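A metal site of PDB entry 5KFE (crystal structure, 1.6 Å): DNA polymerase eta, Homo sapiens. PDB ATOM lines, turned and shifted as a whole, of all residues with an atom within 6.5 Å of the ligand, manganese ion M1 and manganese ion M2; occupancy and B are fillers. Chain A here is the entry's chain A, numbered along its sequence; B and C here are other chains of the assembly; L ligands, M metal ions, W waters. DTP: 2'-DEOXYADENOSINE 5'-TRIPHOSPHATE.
N3 of DT 8 of chain B is in hydrogen-bond range of N6 of the ligand, at 3.4 Å.
The side-chain hydroxyl (OH) of Tyr 55 lies within hydrogen-bond range of an oxygen (O2G) of the ligand (2.6 Å).
An oxygen (O1G) of the ligand lies within salt-bridge range of the side-chain amino group of Lys 234, 2.7 Å away.
O4 of DT 4 of chain C sits at hydrogen-bond distance from N6 of the ligand (3.0 Å).
An oxygen (O1G) of the ligand lies within salt-bridge range of the guanidinium group (NH1) of Arg 58, at 3.0 Å.
The backbone NH (N) of Cys 19 is in hydrogen-bond range of an oxygen (O2G) of the ligand (2.9 Å).
N of Phe 20 lies within hydrogen-bond range of O2B of the ligand, at 3.5 Å.
N of Phe 21 sits at hydrogen-bond distance from O3' of the ligand (3.1 Å).
O2B of the ligand is in salt-bridge range of NH2 of Arg 64 (3.2 Å).
The side-chain hydroxyl (OG) of Ser 116 sits at hydrogen-bond distance from the backbone NH (N) of Asp 118, at 3.0 Å.
The side-chain hydroxyl of Ser 116 is in hydrogen-bond range of the backbone NH of Glu 119, at 3.2 Å.
NZ of Lys 227 lies close to OD2 of Asp 16 (3.96 Å).
NZ of Lys 227 lies within salt-bridge range of OP1 of DT 8 of chain B (3.98 Å).
O2 of DT 4 of chain C lies within hydrogen-bond range of the side-chain amide nitrogen of Gln 41 (2.8 Å).
The guanidinium group of Arg 58 lies within hydrogen-bond range of the backbone carbonyl oxygen of Val 53 (2.9 Å).
The backbone carbonyl oxygen (O) of Ile 51 sits at hydrogen-bond distance from the guanidinium group (NE) of Arg 64, 3.0 Å away.
The side-chain carboxylate (OD1) of Asp 18 sits at hydrogen-bond distance from the side-chain hydroxyl (OG) of Ser 216 (2.9 Å).
N1 of DA 5 of chain C sits close to a nitrogen (N1) of the ligand (3.5 Å).
Merely in contact with the ligand: Ile 51, Asp 18, Ala 52 and Ile 117.
Hydrophobic or aromatic side chains within 4 Å of the ligand: Phe 20, Phe 21, Ile 51, Ala 52, Tyr 55 and Ile 117.
Along chain A the residues within 4 Å of the ligand span positions 16 to 234.
Of the 27 residues printed, 3 come within 4 Å of manganese ion M1.
The nearest printed residue that does not touch manganese ion M1 is Asp 18 (4.4 Å).
OG of Ser 116 touches manganese ion M2, at 3.8 Å.
Within 4 Å of manganese ion M2: Asp 16, Ser 116, Asp 118, Glu 119 and DT 8 of chain B.
The nearest printed residue that does not touch manganese ion M2 is Lys 227 (4.2 Å).
Manganese ion M1 is bound by the side-chain carboxylate of Asp 118, the backbone carbonyl oxygen of Met 17, an oxygen (O1B) of the ligand, the side-chain carboxylate of Asp 16, an oxygen (O3G) of the ligand and an oxygen (O2A) of the ligand.
Manganese ion M2 is bound by OD1 of Asp 118 (2.1 Å), OE2 of Glu 119 (2.1 Å), water W4 (2.2 Å), O2A of the ligand (2.2 Å), OD2 of Asp 16 (2.2 Å) and O3' of DT 8 of chain B (2.3 Å).
Water W4 bridges the side-chain amino group (NZ) of Lys 227 and an oxygen (O1A) of the ligand.
Water W7 lies within hydrogen-bond range of O2 of DT 8 of chain B (2.8 Å) and an oxygen (O4') of the ligand (3.5 Å).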
ATOM      1  N   ASP A  16     -27.180 -28.196 -14.059  1.00  0.00           N
ATOM      2  CA  ASP A  16     -26.705 -27.990 -12.707  1.00  0.00           C
ATOM      3  C   ASP A  16     -25.285 -28.512 -12.494  1.00  0.00           C
ATOM      4  O   ASP A  16     -25.039 -29.601 -12.770  1.00  0.00           O
ATOM      5  CB  ASP A  16     -27.593 -28.717 -11.735  1.00  0.00           C
ATOM      6  CG  ASP A  16     -27.253 -28.457 -10.336  1.00  0.00           C
ATOM      7  OD1 ASP A  16     -26.546 -29.189  -9.801  1.00  0.00           O
ATOM      8  OD2 ASP A  16     -27.802 -27.552  -9.821  1.00  0.00           O
ATOM      9  N   MET A  17     -24.414 -27.676 -11.997  1.00  0.00           N
ATOM     10  CA  MET A  17     -23.013 -28.106 -11.878  1.00  0.00           C
ATOM     11  C   MET A  17     -22.828 -29.223 -10.846  1.00  0.00           C
ATOM     12  O   MET A  17     -23.508 -29.239  -9.835  1.00  0.00           O
ATOM     13  CB  MET A  17     -22.126 -26.906 -11.497  1.00  0.00           C
ATOM     14  CG  MET A  17     -22.269 -25.725 -12.429  1.00  0.00           C
ATOM     15  SD  MET A  17     -22.048 -26.113 -14.180  1.00  0.00           S
ATOM     16  CE  MET A  17     -20.358 -26.612 -14.201  1.00  0.00           C
ATOM     17  N   ASP A  18     -21.947 -30.175 -11.087  1.00  0.00           N
ATOM     18  CA  ASP A  18     -21.687 -31.224 -10.112  1.00  0.00           C
ATOM     19  C   ASP A  18     -20.809 -30.655  -8.993  1.00  0.00           C
ATOM     20  O   ASP A  18     -19.865 -29.994  -9.262  1.00  0.00           O
ATOM     21  CB  ASP A  18     -20.989 -32.390 -10.773  1.00  0.00           C
ATOM     22  CG  ASP A  18     -21.848 -33.089 -11.835  1.00  0.00           C
ATOM     23  OD1 ASP A  18     -23.053 -32.973 -11.804  1.00  0.00           O
ATOM     24  OD2 ASP A  18     -21.281 -33.742 -12.622  1.00  0.00           O
ATOM     25  N   CYS A  19     -21.183 -30.956  -7.756  1.00  0.00           N
ATOM     26  CA  CYS A  19     -20.471 -30.531  -6.533  1.00  0.00           C
ATOM     27  C   CYS A  19     -19.681 -29.237  -6.795  1.00  0.00           C
ATOM     28  O   CYS A  19     -18.448 -29.211  -6.720  1.00  0.00           O
ATOM     29  CB  CYS A  19     -19.555 -31.640  -5.988  1.00  0.00           C
ATOM     30  SG  CYS A  19     -18.394 -32.448  -7.102  1.00  0.00           S
ATOM     31  N   PHE A  20     -20.405 -28.164  -7.114  1.00  0.00           N
ATOM     32  CA  PHE A  20     -19.823 -27.005  -7.783  1.00  0.00           C
ATOM     33  C   PHE A  20     -18.615 -26.378  -7.082  1.00  0.00           C
ATOM     34  O   PHE A  20     -17.558 -26.252  -7.696  1.00  0.00           O
ATOM     35  CB  PHE A  20     -20.892 -25.924  -8.018  1.00  0.00           C
ATOM     36  CG  PHE A  20     -20.392 -24.750  -8.825  1.00  0.00           C
ATOM     37  CD1 PHE A  20     -19.632 -24.953  -9.963  1.00  0.00           C
ATOM     38  CD2 PHE A  20     -20.705 -23.451  -8.438  1.00  0.00           C
ATOM     39  CE1 PHE A  20     -19.185 -23.848 -10.721  1.00  0.00           C
ATOM     40  CE2 PHE A  20     -20.265 -22.362  -9.198  1.00  0.00           C
ATOM     41  CZ  PHE A  20     -19.506 -22.559 -10.328  1.00  0.00           C
ATOM     42  N   PHE A  21     -18.759 -25.976  -5.821  1.00  0.00           N
ATOM     43  CA  PHE A  21     -17.642 -25.280  -5.163  1.00  0.00           C
ATOM     44  C   PHE A  21     -16.416 -26.196  -5.085  1.00  0.00           C
ATOM     45  O   PHE A  21     -15.281 -25.731  -5.142  1.00  0.00           O
ATOM     46  CB  PHE A  21     -18.008 -24.776  -3.758  1.00  0.00           C
ATOM     47  CG  PHE A  21     -18.969 -23.623  -3.724  1.00  0.00           C
ATOM     48  CD1 PHE A  21     -19.704 -23.217  -4.841  1.00  0.00           C
ATOM     49  CD2 PHE A  21     -19.156 -22.941  -2.532  1.00  0.00           C
ATOM     50  CE1 PHE A  21     -20.605 -22.142  -4.752  1.00  0.00           C
ATOM     51  CE2 PHE A  21     -20.037 -21.863  -2.441  1.00  0.00           C
ATOM     52  CZ  PHE A  21     -20.770 -21.473  -3.547  1.00  0.00           C
ATOM     53  N   VAL A  22     -16.646 -27.508  -4.906  1.00  0.00           N
ATOM     54  CA  VAL A  22     -15.541 -28.457  -4.905  1.00  0.00           C
ATOM     55  C   VAL A  22     -14.837 -28.467  -6.265  1.00  0.00           C
ATOM     56  O   VAL A  22     -13.596 -28.433  -6.318  1.00  0.00           O
ATOM     57  CB  VAL A  22     -16.033 -29.869  -4.548  1.00  0.00           C
ATOM     58  CG1 VAL A  22     -14.989 -30.939  -4.909  1.00  0.00           C
ATOM     59  CG2 VAL A  22     -16.405 -29.949  -3.058  1.00  0.00           C
ATOM     60  N   GLN A  41     -16.478 -23.528   5.392  1.00  0.00           N
ATOM     61  CA  GLN A  41     -16.348 -22.125   5.748  1.00  0.00           C
ATOM     62  C   GLN A  41     -16.102 -22.015   7.245  1.00  0.00           C
ATOM     63  O   GLN A  41     -16.725 -22.714   8.041  1.00  0.00           O
ATOM     64  CB  GLN A  41     -17.550 -21.292   5.312  1.00  0.00           C
ATOM     65  CG  GLN A  41     -18.894 -21.823   5.706  1.00  0.00           C
ATOM     66  CD  GLN A  41     -20.015 -21.088   4.985  1.00  0.00           C
ATOM     67  OE1 GLN A  41     -19.777 -20.329   4.043  1.00  0.00           O
ATOM     68  NE2 GLN A  41     -21.235 -21.305   5.431  1.00  0.00           N
ATOM     69  N   ILE A  51     -19.969 -26.962   3.057  1.00  0.00           N
ATOM     70  CA  ILE A  51     -21.012 -26.469   2.162  1.00  0.00           C
ATOM     71  C   ILE A  51     -21.003 -27.155   0.788  1.00  0.00           C
ATOM     72  O   ILE A  51     -21.930 -26.972   0.010  1.00  0.00           O
ATOM     73  CB  ILE A  51     -20.920 -24.937   1.949  1.00  0.00           C
ATOM     74  CG1 ILE A  51     -19.562 -24.520   1.379  1.00  0.00           C
ATOM     75  CG2 ILE A  51     -21.217 -24.218   3.279  1.00  0.00           C
ATOM     76  CD1 ILE A  51     -19.511 -23.030   1.013  1.00  0.00           C
ATOM     77  N   ALA A  52     -19.989 -27.971   0.491  1.00  0.00           N
ATOM     78  CA  ALA A  52     -19.965 -28.732  -0.767  1.00  0.00           C
ATOM     79  C   ALA A  52     -19.097 -29.971  -0.598  1.00  0.00           C
ATOM     80  O   ALA A  52     -18.105 -29.931   0.135  1.00  0.00           O
ATOM     81  CB  ALA A  52     -19.454 -27.861  -1.942  1.00  0.00           C
ATOM     82  N   VAL A  53     -19.471 -31.065  -1.258  1.00  0.00           N
ATOM     83  CA  VAL A  53     -18.862 -32.373  -1.021  1.00  0.00           C
ATOM     84  C   VAL A  53     -18.642 -33.124  -2.331  1.00  0.00           C
ATOM     85  O   VAL A  53     -19.601 -33.284  -3.097  1.00  0.00           O
ATOM     86  CB  VAL A  53     -19.758 -33.253  -0.104  1.00  0.00           C
ATOM     87  CG1 VAL A  53     -19.045 -34.531   0.294  1.00  0.00           C
ATOM     88  CG2 VAL A  53     -20.197 -32.495   1.132  1.00  0.00           C
ATOM     89  N   TYR A  55     -18.090 -36.339  -4.868  1.00  0.00           N
ATOM     90  CA  TYR A  55     -18.822 -37.606  -4.886  1.00  0.00           C
ATOM     91  C   TYR A  55     -18.027 -38.723  -4.211  1.00  0.00           C
ATOM     92  O   TYR A  55     -18.614 -39.606  -3.588  1.00  0.00           O
ATOM     93  CB  TYR A  55     -19.224 -37.960  -6.318  1.00  0.00           C
ATOM     94  CG  TYR A  55     -20.443 -37.157  -6.723  1.00  0.00           C
ATOM     95  CD1 TYR A  55     -20.326 -35.840  -7.151  1.00  0.00           C
ATOM     96  CD2 TYR A  55     -21.713 -37.697  -6.593  1.00  0.00           C
ATOM     97  CE1 TYR A  55     -21.432 -35.087  -7.473  1.00  0.00           C
ATOM     98  CE2 TYR A  55     -22.838 -36.955  -6.911  1.00  0.00           C
ATOM     99  CZ  TYR A  55     -22.696 -35.655  -7.348  1.00  0.00           C
ATOM    100  OH  TYR A  55     -23.827 -34.937  -7.663  1.00  0.00           O
ATOM    101  N   ARG A  58     -18.884 -38.246  -0.609  1.00  0.00           N
ATOM    102  CA  ARG A  58     -20.263 -38.643  -0.317  1.00  0.00           C
ATOM    103  C   ARG A  58     -20.385 -40.145  -0.057  1.00  0.00           C
ATOM    104  O   ARG A  58     -21.250 -40.566   0.717  1.00  0.00           O
ATOM    105  CB  ARG A  58     -21.199 -38.242  -1.460  1.00  0.00           C
ATOM    106  CG  ARG A  58     -21.237 -36.768  -1.696  1.00  0.00           C
ATOM    107  CD  ARG A  58     -22.223 -36.401  -2.776  1.00  0.00           C
ATOM    108  NE  ARG A  58     -21.964 -35.023  -3.194  1.00  0.00           N
ATOM    109  CZ  ARG A  58     -22.773 -34.301  -3.965  1.00  0.00           C
ATOM    110  NH1 ARG A  58     -23.922 -34.808  -4.391  1.00  0.00           N
ATOM    111  NH2 ARG A  58     -22.421 -33.038  -4.283  1.00  0.00           N
ATOM    112  N   ARG A  64     -23.365 -31.933   3.157  1.00  0.00           N
ATOM    113  CA  ARG A  64     -23.507 -30.523   3.465  1.00  0.00           C
ATOM    114  C   ARG A  64     -24.080 -30.358   4.879  1.00  0.00           C
ATOM    115  O   ARG A  64     -24.820 -31.224   5.346  1.00  0.00           O
ATOM    116  CB  ARG A  64     -24.403 -29.864   2.397  1.00  0.00           C
ATOM    117  CG  ARG A  64     -24.930 -28.478   2.716  1.00  0.00           C
ATOM    118  CD  ARG A  64     -25.669 -27.939   1.493  1.00  0.00           C
ATOM    119  NE  ARG A  64     -24.733 -27.879   0.380  1.00  0.00           N
ATOM    120  CZ  ARG A  64     -24.958 -28.350  -0.848  1.00  0.00           C
ATOM    121  NH1 ARG A  64     -26.113 -28.924  -1.178  1.00  0.00           N
ATOM    122  NH2 ARG A  64     -24.005 -28.245  -1.765  1.00  0.00           N
ATOM    123  N   LEU A  92     -17.641 -15.141  -1.077  1.00  0.00           N
ATOM    124  CA  LEU A  92     -17.930 -16.144  -2.105  1.00  0.00           C
ATOM    125  C   LEU A  92     -17.573 -15.721  -3.530  1.00  0.00           C
ATOM    126  O   LEU A  92     -18.028 -16.328  -4.498  1.00  0.00           O
ATOM    127  CB  LEU A  92     -19.415 -16.532  -2.039  1.00  0.00           C
ATOM    128  CG  LEU A  92     -19.893 -16.944  -0.647  1.00  0.00           C
ATOM    129  CD1 LEU A  92     -21.391 -17.168  -0.661  1.00  0.00           C
ATOM    130  CD2 LEU A  92     -19.146 -18.200  -0.207  1.00  0.00           C
ATOM    131  N   SER A 116     -29.737 -20.411  -9.604  1.00  0.00           N
ATOM    132  CA  SER A 116     -28.882 -20.433  -8.422  1.00  0.00           C
ATOM    133  C   SER A 116     -27.456 -20.112  -8.861  1.00  0.00           C
ATOM    134  O   SER A 116     -27.202 -19.909 -10.042  1.00  0.00           O
ATOM    135  CB  SER A 116     -28.902 -21.789  -7.722  1.00  0.00           C
ATOM    136  OG  SER A 116     -28.034 -22.715  -8.368  1.00  0.00           O
ATOM    137  N   ILE A 117     -26.522 -20.124  -7.918  1.00  0.00           N
ATOM    138  CA  ILE A 117     -25.139 -19.881  -8.287  1.00  0.00           C
ATOM    139  C   ILE A 117     -24.604 -20.974  -9.231  1.00  0.00           C
ATOM    140  O   ILE A 117     -23.636 -20.761  -9.949  1.00  0.00           O
ATOM    141  CB  ILE A 117     -24.254 -19.775  -7.002  1.00  0.00           C
ATOM    142  CG1 ILE A 117     -22.931 -19.098  -7.329  1.00  0.00           C
ATOM    143  CG2 ILE A 117     -24.062 -21.153  -6.368  1.00  0.00           C
ATOM    144  CD1 ILE A 117     -22.164 -18.662  -6.065  1.00  0.00           C
ATOM    145  N   ASP A 118     -25.229 -22.154  -9.250  1.00  0.00           N
ATOM    146  CA  ASP A 118     -24.667 -23.227 -10.067  1.00  0.00           C
ATOM    147  C   ASP A 118     -25.643 -23.882 -11.034  1.00  0.00           C
ATOM    148  O   ASP A 118     -25.378 -24.975 -11.539  1.00  0.00           O
ATOM    149  CB  ASP A 118     -24.037 -24.316  -9.173  1.00  0.00           C
ATOM    150  CG  ASP A 118     -25.024 -25.419  -8.788  1.00  0.00           C
ATOM    151  OD1 ASP A 118     -26.217 -25.158  -8.473  1.00  0.00           O
ATOM    152  OD2 ASP A 118     -24.583 -26.605  -8.869  1.00  0.00           O
ATOM    153  N   GLU A 119     -26.775 -23.228 -11.317  1.00  0.00           N
ATOM    154  CA  GLU A 119     -27.715 -23.815 -12.263  1.00  0.00           C
ATOM    155  C   GLU A 119     -28.558 -22.807 -12.994  1.00  0.00           C
ATOM    156  O   GLU A 119     -28.805 -21.695 -12.500  1.00  0.00           O
ATOM    157  CB  GLU A 119     -28.634 -24.818 -11.562  1.00  0.00           C
ATOM    158  CG  GLU A 119     -29.730 -24.195 -10.714  1.00  0.00           C
ATOM    159  CD  GLU A 119     -30.108 -25.115  -9.577  1.00  0.00           C
ATOM    160  OE1 GLU A 119     -31.138 -25.813  -9.670  1.00  0.00           O
ATOM    161  OE2 GLU A 119     -29.344 -25.166  -8.591  1.00  0.00           O
ATOM    162  N   SER A 216     -24.559 -31.899 -14.663  1.00  0.00           N
ATOM    163  CA  SER A 216     -25.643 -32.793 -15.052  1.00  0.00           C
ATOM    164  C   SER A 216     -26.753 -31.956 -15.632  1.00  0.00           C
ATOM    165  O   SER A 216     -26.722 -30.743 -15.523  1.00  0.00           O
ATOM    166  CB  SER A 216     -26.119 -33.590 -13.848  1.00  0.00           C
ATOM    167  OG  SER A 216     -25.056 -34.406 -13.367  1.00  0.00           O
ATOM    168  N   LYS A 227     -35.888 -29.982 -13.718  1.00  0.00           N
ATOM    169  CA  LYS A 227     -35.138 -30.014 -12.464  1.00  0.00           C
ATOM    170  C   LYS A 227     -35.143 -31.419 -11.851  1.00  0.00           C
ATOM    171  O   LYS A 227     -34.106 -31.900 -11.400  1.00  0.00           O
ATOM    172  CB  LYS A 227     -35.726 -28.997 -11.464  1.00  0.00           C
ATOM    173  CG  LYS A 227     -35.046 -29.039 -10.093  1.00  0.00           C
ATOM    174  CD  LYS A 227     -33.550 -28.717 -10.149  1.00  0.00           C
ATOM    175  CE  LYS A 227     -32.949 -28.729  -8.741  1.00  0.00           C
ATOM    176  NZ  LYS A 227     -31.512 -28.307  -8.667  1.00  0.00           N
ATOM    177  N   LYS A 234     -27.149 -37.993 -11.641  1.00  0.00           N
ATOM    178  CA  LYS A 234     -25.879 -37.304 -11.342  1.00  0.00           C
ATOM    179  C   LYS A 234     -24.790 -38.242 -10.795  1.00  0.00           C
ATOM    180  O   LYS A 234     -25.132 -39.179 -10.183  1.00  0.00           O
ATOM    181  CB  LYS A 234     -26.164 -36.122 -10.421  1.00  0.00           C
ATOM    182  CG  LYS A 234     -26.968 -36.487  -9.253  1.00  0.00           C
ATOM    183  CD  LYS A 234     -27.275 -35.272  -8.385  1.00  0.00           C
ATOM    184  CE  LYS A 234     -26.994 -35.574  -6.914  1.00  0.00           C
ATOM    185  NZ  LYS A 234     -27.392 -34.386  -6.119  1.00  0.00           N
ATOM    186  N   PRO A 235     -23.506 -37.943 -10.951  1.00  0.00           N
ATOM    187  CA  PRO A 235     -22.987 -36.756 -11.640  1.00  0.00           C
ATOM    188  C   PRO A 235     -22.649 -37.016 -13.097  1.00  0.00           C
ATOM    189  O   PRO A 235     -22.632 -38.172 -13.546  1.00  0.00           O
ATOM    190  CB  PRO A 235     -21.707 -36.463 -10.863  1.00  0.00           C
ATOM    191  CG  PRO A 235     -21.193 -37.848 -10.529  1.00  0.00           C
ATOM    192  CD  PRO A 235     -22.436 -38.706 -10.295  1.00  0.00           C
ATOM    193  P    DT B   8     -33.034 -26.846  -3.910  1.00  0.00           P
ATOM    194  OP1  DT B   8     -33.055 -27.821  -5.027  1.00  0.00           O
ATOM    195  OP2  DT B   8     -32.890 -27.324  -2.505  1.00  0.00           O
ATOM    196  O5'  DT B   8     -31.863 -25.764  -4.131  1.00  0.00           O
ATOM    197  C5'  DT B   8     -31.569 -25.096  -5.431  1.00  0.00           C
ATOM    198  C4'  DT B   8     -30.226 -24.404  -5.294  1.00  0.00           C
ATOM    199  O4'  DT B   8     -30.351 -23.617  -4.087  1.00  0.00           O
ATOM    200  C3'  DT B   8     -29.135 -25.446  -5.044  1.00  0.00           C
ATOM    201  O3'  DT B   8     -28.016 -25.210  -5.909  1.00  0.00           O
ATOM    202  C2'  DT B   8     -28.768 -25.260  -3.563  1.00  0.00           C
ATOM    203  C1'  DT B   8     -29.218 -23.833  -3.269  1.00  0.00           C
ATOM    204  N1   DT B   8     -29.599 -23.604  -1.848  1.00  0.00           N
ATOM    205  C2   DT B   8     -28.919 -22.652  -1.126  1.00  0.00           C
ATOM    206  O2   DT B   8     -28.022 -21.984  -1.583  1.00  0.00           O
ATOM    207  N3   DT B   8     -29.335 -22.520   0.183  1.00  0.00           N
ATOM    208  C4   DT B   8     -30.333 -23.213   0.811  1.00  0.00           C
ATOM    209  O4   DT B   8     -30.625 -23.023   1.992  1.00  0.00           O
ATOM    210  C5   DT B   8     -31.009 -24.202   0.003  1.00  0.00           C
ATOM    211  C7   DT B   8     -32.123 -25.027   0.587  1.00  0.00           C
ATOM    212  C6   DT B   8     -30.615 -24.342  -1.280  1.00  0.00           C
ATOM    213  P    DT C   3     -26.138 -25.969  14.854  1.00  0.00           P
ATOM    214  OP1  DT C   3     -27.408 -25.513  15.449  1.00  0.00           O
ATOM    215  OP2  DT C   3     -25.615 -27.321  15.129  1.00  0.00           O
ATOM    216  O5'  DT C   3     -26.243 -25.796  13.262  1.00  0.00           O
ATOM    217  C5'  DT C   3     -25.089 -25.898  12.455  1.00  0.00           C
ATOM    218  C4'  DT C   3     -25.369 -25.404  11.060  1.00  0.00           C
ATOM    219  O4'  DT C   3     -26.063 -26.436  10.316  1.00  0.00           O
ATOM    220  C3'  DT C   3     -26.258 -24.158  11.007  1.00  0.00           C
ATOM    221  O3'  DT C   3     -25.571 -23.086  10.371  1.00  0.00           O
ATOM    222  C2'  DT C   3     -27.501 -24.602  10.221  1.00  0.00           C
ATOM    223  C1'  DT C   3     -27.017 -25.840   9.479  1.00  0.00           C
ATOM    224  N1   DT C   3     -28.083 -26.831   9.211  1.00  0.00           N
ATOM    225  C2   DT C   3     -28.376 -27.172   7.916  1.00  0.00           C
ATOM    226  O2   DT C   3     -27.792 -26.694   6.958  1.00  0.00           O
ATOM    227  N3   DT C   3     -29.372 -28.097   7.778  1.00  0.00           N
ATOM    228  C4   DT C   3     -30.091 -28.706   8.801  1.00  0.00           C
ATOM    229  O4   DT C   3     -30.967 -29.529   8.579  1.00  0.00           O
ATOM    230  C5   DT C   3     -29.732 -28.301  10.139  1.00  0.00           C
ATOM    231  C7   DT C   3     -30.448 -28.883  11.317  1.00  0.00           C
ATOM    232  C6   DT C   3     -28.754 -27.387  10.281  1.00  0.00           C
ATOM    233  P    DT C   4     -25.287 -21.741  11.220  1.00  0.00           P
ATOM    234  OP1  DT C   4     -24.472 -22.103  12.385  1.00  0.00           O
ATOM    235  OP2  DT C   4     -26.599 -21.086  11.396  1.00  0.00           O
ATOM    236  O5'  DT C   4     -24.444 -20.805  10.217  1.00  0.00           O
ATOM    237  C5'  DT C   4     -23.020 -20.919  10.119  1.00  0.00           C
ATOM    238  C4'  DT C   4     -22.553 -20.255   8.821  1.00  0.00           C
ATOM    239  O4'  DT C   4     -23.115 -21.007   7.722  1.00  0.00           O
ATOM    240  C3'  DT C   4     -23.047 -18.826   8.646  1.00  0.00           C
ATOM    241  O3'  DT C   4     -22.049 -18.100   7.945  1.00  0.00           O
ATOM    242  C2'  DT C   4     -24.322 -19.005   7.803  1.00  0.00           C
ATOM    243  C1'  DT C   4     -23.904 -20.151   6.909  1.00  0.00           C
ATOM    244  N1   DT C   4     -24.984 -20.989   6.358  1.00  0.00           N
ATOM    245  C2   DT C   4     -24.807 -21.464   5.093  1.00  0.00           C
ATOM    246  O2   DT C   4     -23.845 -21.169   4.402  1.00  0.00           O
ATOM    247  N3   DT C   4     -25.810 -22.267   4.645  1.00  0.00           N
ATOM    248  C4   DT C   4     -26.935 -22.673   5.330  1.00  0.00           C
ATOM    249  O4   DT C   4     -27.771 -23.413   4.822  1.00  0.00           O
ATOM    250  C5   DT C   4     -27.054 -22.156   6.677  1.00  0.00           C
ATOM    251  C7   DT C   4     -28.242 -22.513   7.525  1.00  0.00           C
ATOM    252  C6   DT C   4     -26.062 -21.357   7.138  1.00  0.00           C
ATOM    253  P    DA C   5     -22.253 -16.549   7.584  1.00  0.00           P
ATOM    254  OP1  DA C   5     -20.948 -15.893   7.763  1.00  0.00           O
ATOM    255  OP2  DA C   5     -23.459 -16.047   8.284  1.00  0.00           O
ATOM    256  O5'  DA C   5     -22.623 -16.575   6.052  1.00  0.00           O
ATOM    257  C5'  DA C   5     -21.640 -16.969   5.093  1.00  0.00           C
ATOM    258  C4'  DA C   5     -22.188 -16.803   3.700  1.00  0.00           C
ATOM    259  O4'  DA C   5     -23.236 -17.787   3.456  1.00  0.00           O
ATOM    260  C3'  DA C   5     -22.814 -15.441   3.421  1.00  0.00           C
ATOM    261  O3'  DA C   5     -22.499 -15.058   2.102  1.00  0.00           O
ATOM    262  C2'  DA C   5     -24.307 -15.717   3.592  1.00  0.00           C
ATOM    263  C1'  DA C   5     -24.386 -17.121   2.988  1.00  0.00           C
ATOM    264  N9   DA C   5     -25.548 -17.884   3.408  1.00  0.00           N
ATOM    265  C8   DA C   5     -26.161 -17.864   4.630  1.00  0.00           C
ATOM    266  N7   DA C   5     -27.172 -18.698   4.722  1.00  0.00           N
ATOM    267  C5   DA C   5     -27.228 -19.301   3.474  1.00  0.00           C
ATOM    268  C6   DA C   5     -28.092 -20.272   2.925  1.00  0.00           C
ATOM    269  N6   DA C   5     -29.099 -20.824   3.612  1.00  0.00           N
ATOM    270  N1   DA C   5     -27.870 -20.650   1.650  1.00  0.00           N
ATOM    271  C2   DA C   5     -26.853 -20.100   0.978  1.00  0.00           C
ATOM    272  N3   DA C   5     -25.981 -19.169   1.383  1.00  0.00           N
ATOM    273  C4   DA C   5     -26.229 -18.818   2.659  1.00  0.00           C
HETATM  274  PG  DTP L   1     -24.596 -31.620  -6.679  1.00  0.00           P
HETATM  275  O1G DTP L   1     -25.424 -32.573  -5.822  1.00  0.00           O
HETATM  276  O2G DTP L   1     -23.696 -32.360  -7.623  1.00  0.00           O
HETATM  277  O3G DTP L   1     -25.476 -30.636  -7.402  1.00  0.00           O
HETATM  278  PB  DTP L   1     -23.598 -29.244  -5.465  1.00  0.00           P
HETATM  279  O1B DTP L   1     -23.378 -28.548  -6.800  1.00  0.00           O
HETATM  280  O2B DTP L   1     -22.511 -28.937  -4.466  1.00  0.00           O
HETATM  281  O3B DTP L   1     -23.645 -30.838  -5.670  1.00  0.00           O
HETATM  282  PA  DTP L   1     -26.012 -27.706  -5.194  1.00  0.00           P
HETATM  283  O1A DTP L   1     -27.207 -27.927  -4.295  1.00  0.00           O
HETATM  284  O2A DTP L   1     -26.372 -27.705  -6.657  1.00  0.00           O
HETATM  285  O3A DTP L   1     -24.991 -28.872  -4.811  1.00  0.00           O
HETATM  286  O5' DTP L   1     -25.339 -26.350  -4.769  1.00  0.00           O
HETATM  287  C5' DTP L   1     -24.395 -25.676  -5.568  1.00  0.00           C
HETATM  288  C4' DTP L   1     -23.363 -24.942  -4.706  1.00  0.00           C
HETATM  289  O4' DTP L   1     -24.053 -23.978  -3.951  1.00  0.00           O
HETATM  290  C3' DTP L   1     -22.682 -25.826  -3.760  1.00  0.00           C
HETATM  291  O3' DTP L   1     -21.480 -26.374  -4.318  1.00  0.00           O
HETATM  292  C2' DTP L   1     -22.377 -24.970  -2.613  1.00  0.00           C
HETATM  293  C1' DTP L   1     -23.500 -23.971  -2.628  1.00  0.00           C
HETATM  294  N9  DTP L   1     -24.519 -24.289  -1.686  1.00  0.00           N
HETATM  295  C8  DTP L   1     -25.565 -25.145  -1.858  1.00  0.00           C
HETATM  296  N7  DTP L   1     -26.319 -25.189  -0.768  1.00  0.00           N
HETATM  297  C5  DTP L   1     -25.808 -24.349   0.135  1.00  0.00           C
HETATM  298  C6  DTP L   1     -26.154 -23.969   1.432  1.00  0.00           C
HETATM  299  N6  DTP L   1     -27.293 -24.549   2.051  1.00  0.00           N
HETATM  300  N1  DTP L   1     -25.395 -23.085   2.083  1.00  0.00           N
HETATM  301  C2  DTP L   1     -24.299 -22.524   1.531  1.00  0.00           C
HETATM  302  N3  DTP L   1     -23.932 -22.860   0.257  1.00  0.00           N
HETATM  303  C4  DTP L   1     -24.665 -23.755  -0.430  1.00  0.00           C
HETATM  304 MN    MN M   1     -24.961 -28.630  -8.331  1.00  0.00          MN
HETATM  305 MN    MN M   2     -27.798 -26.462  -7.859  1.00  0.00          MN
HETATM  306  O   HOH W   1     -21.947 -30.748  -2.572  1.00  0.00           O
HETATM  307  O   HOH W   2     -26.212 -32.209  -3.328  1.00  0.00           O
HETATM  308  O   HOH W   3     -28.600 -26.713   0.154  1.00  0.00           O
HETATM  309  O   HOH W   4     -29.194 -27.912  -7.080  1.00  0.00           O
HETATM  310  O   HOH W   5     -22.379 -20.629  -0.394  1.00  0.00           O
HETATM  311  O   HOH W   6     -28.173 -30.578  -7.192  1.00  0.00           O
HETATM  312  O   HOH W   7     -25.630 -21.162  -2.720  1.00  0.00           O
HETATM  313  O   HOH W   8     -26.596 -23.228  -5.136  1.00  0.00           O
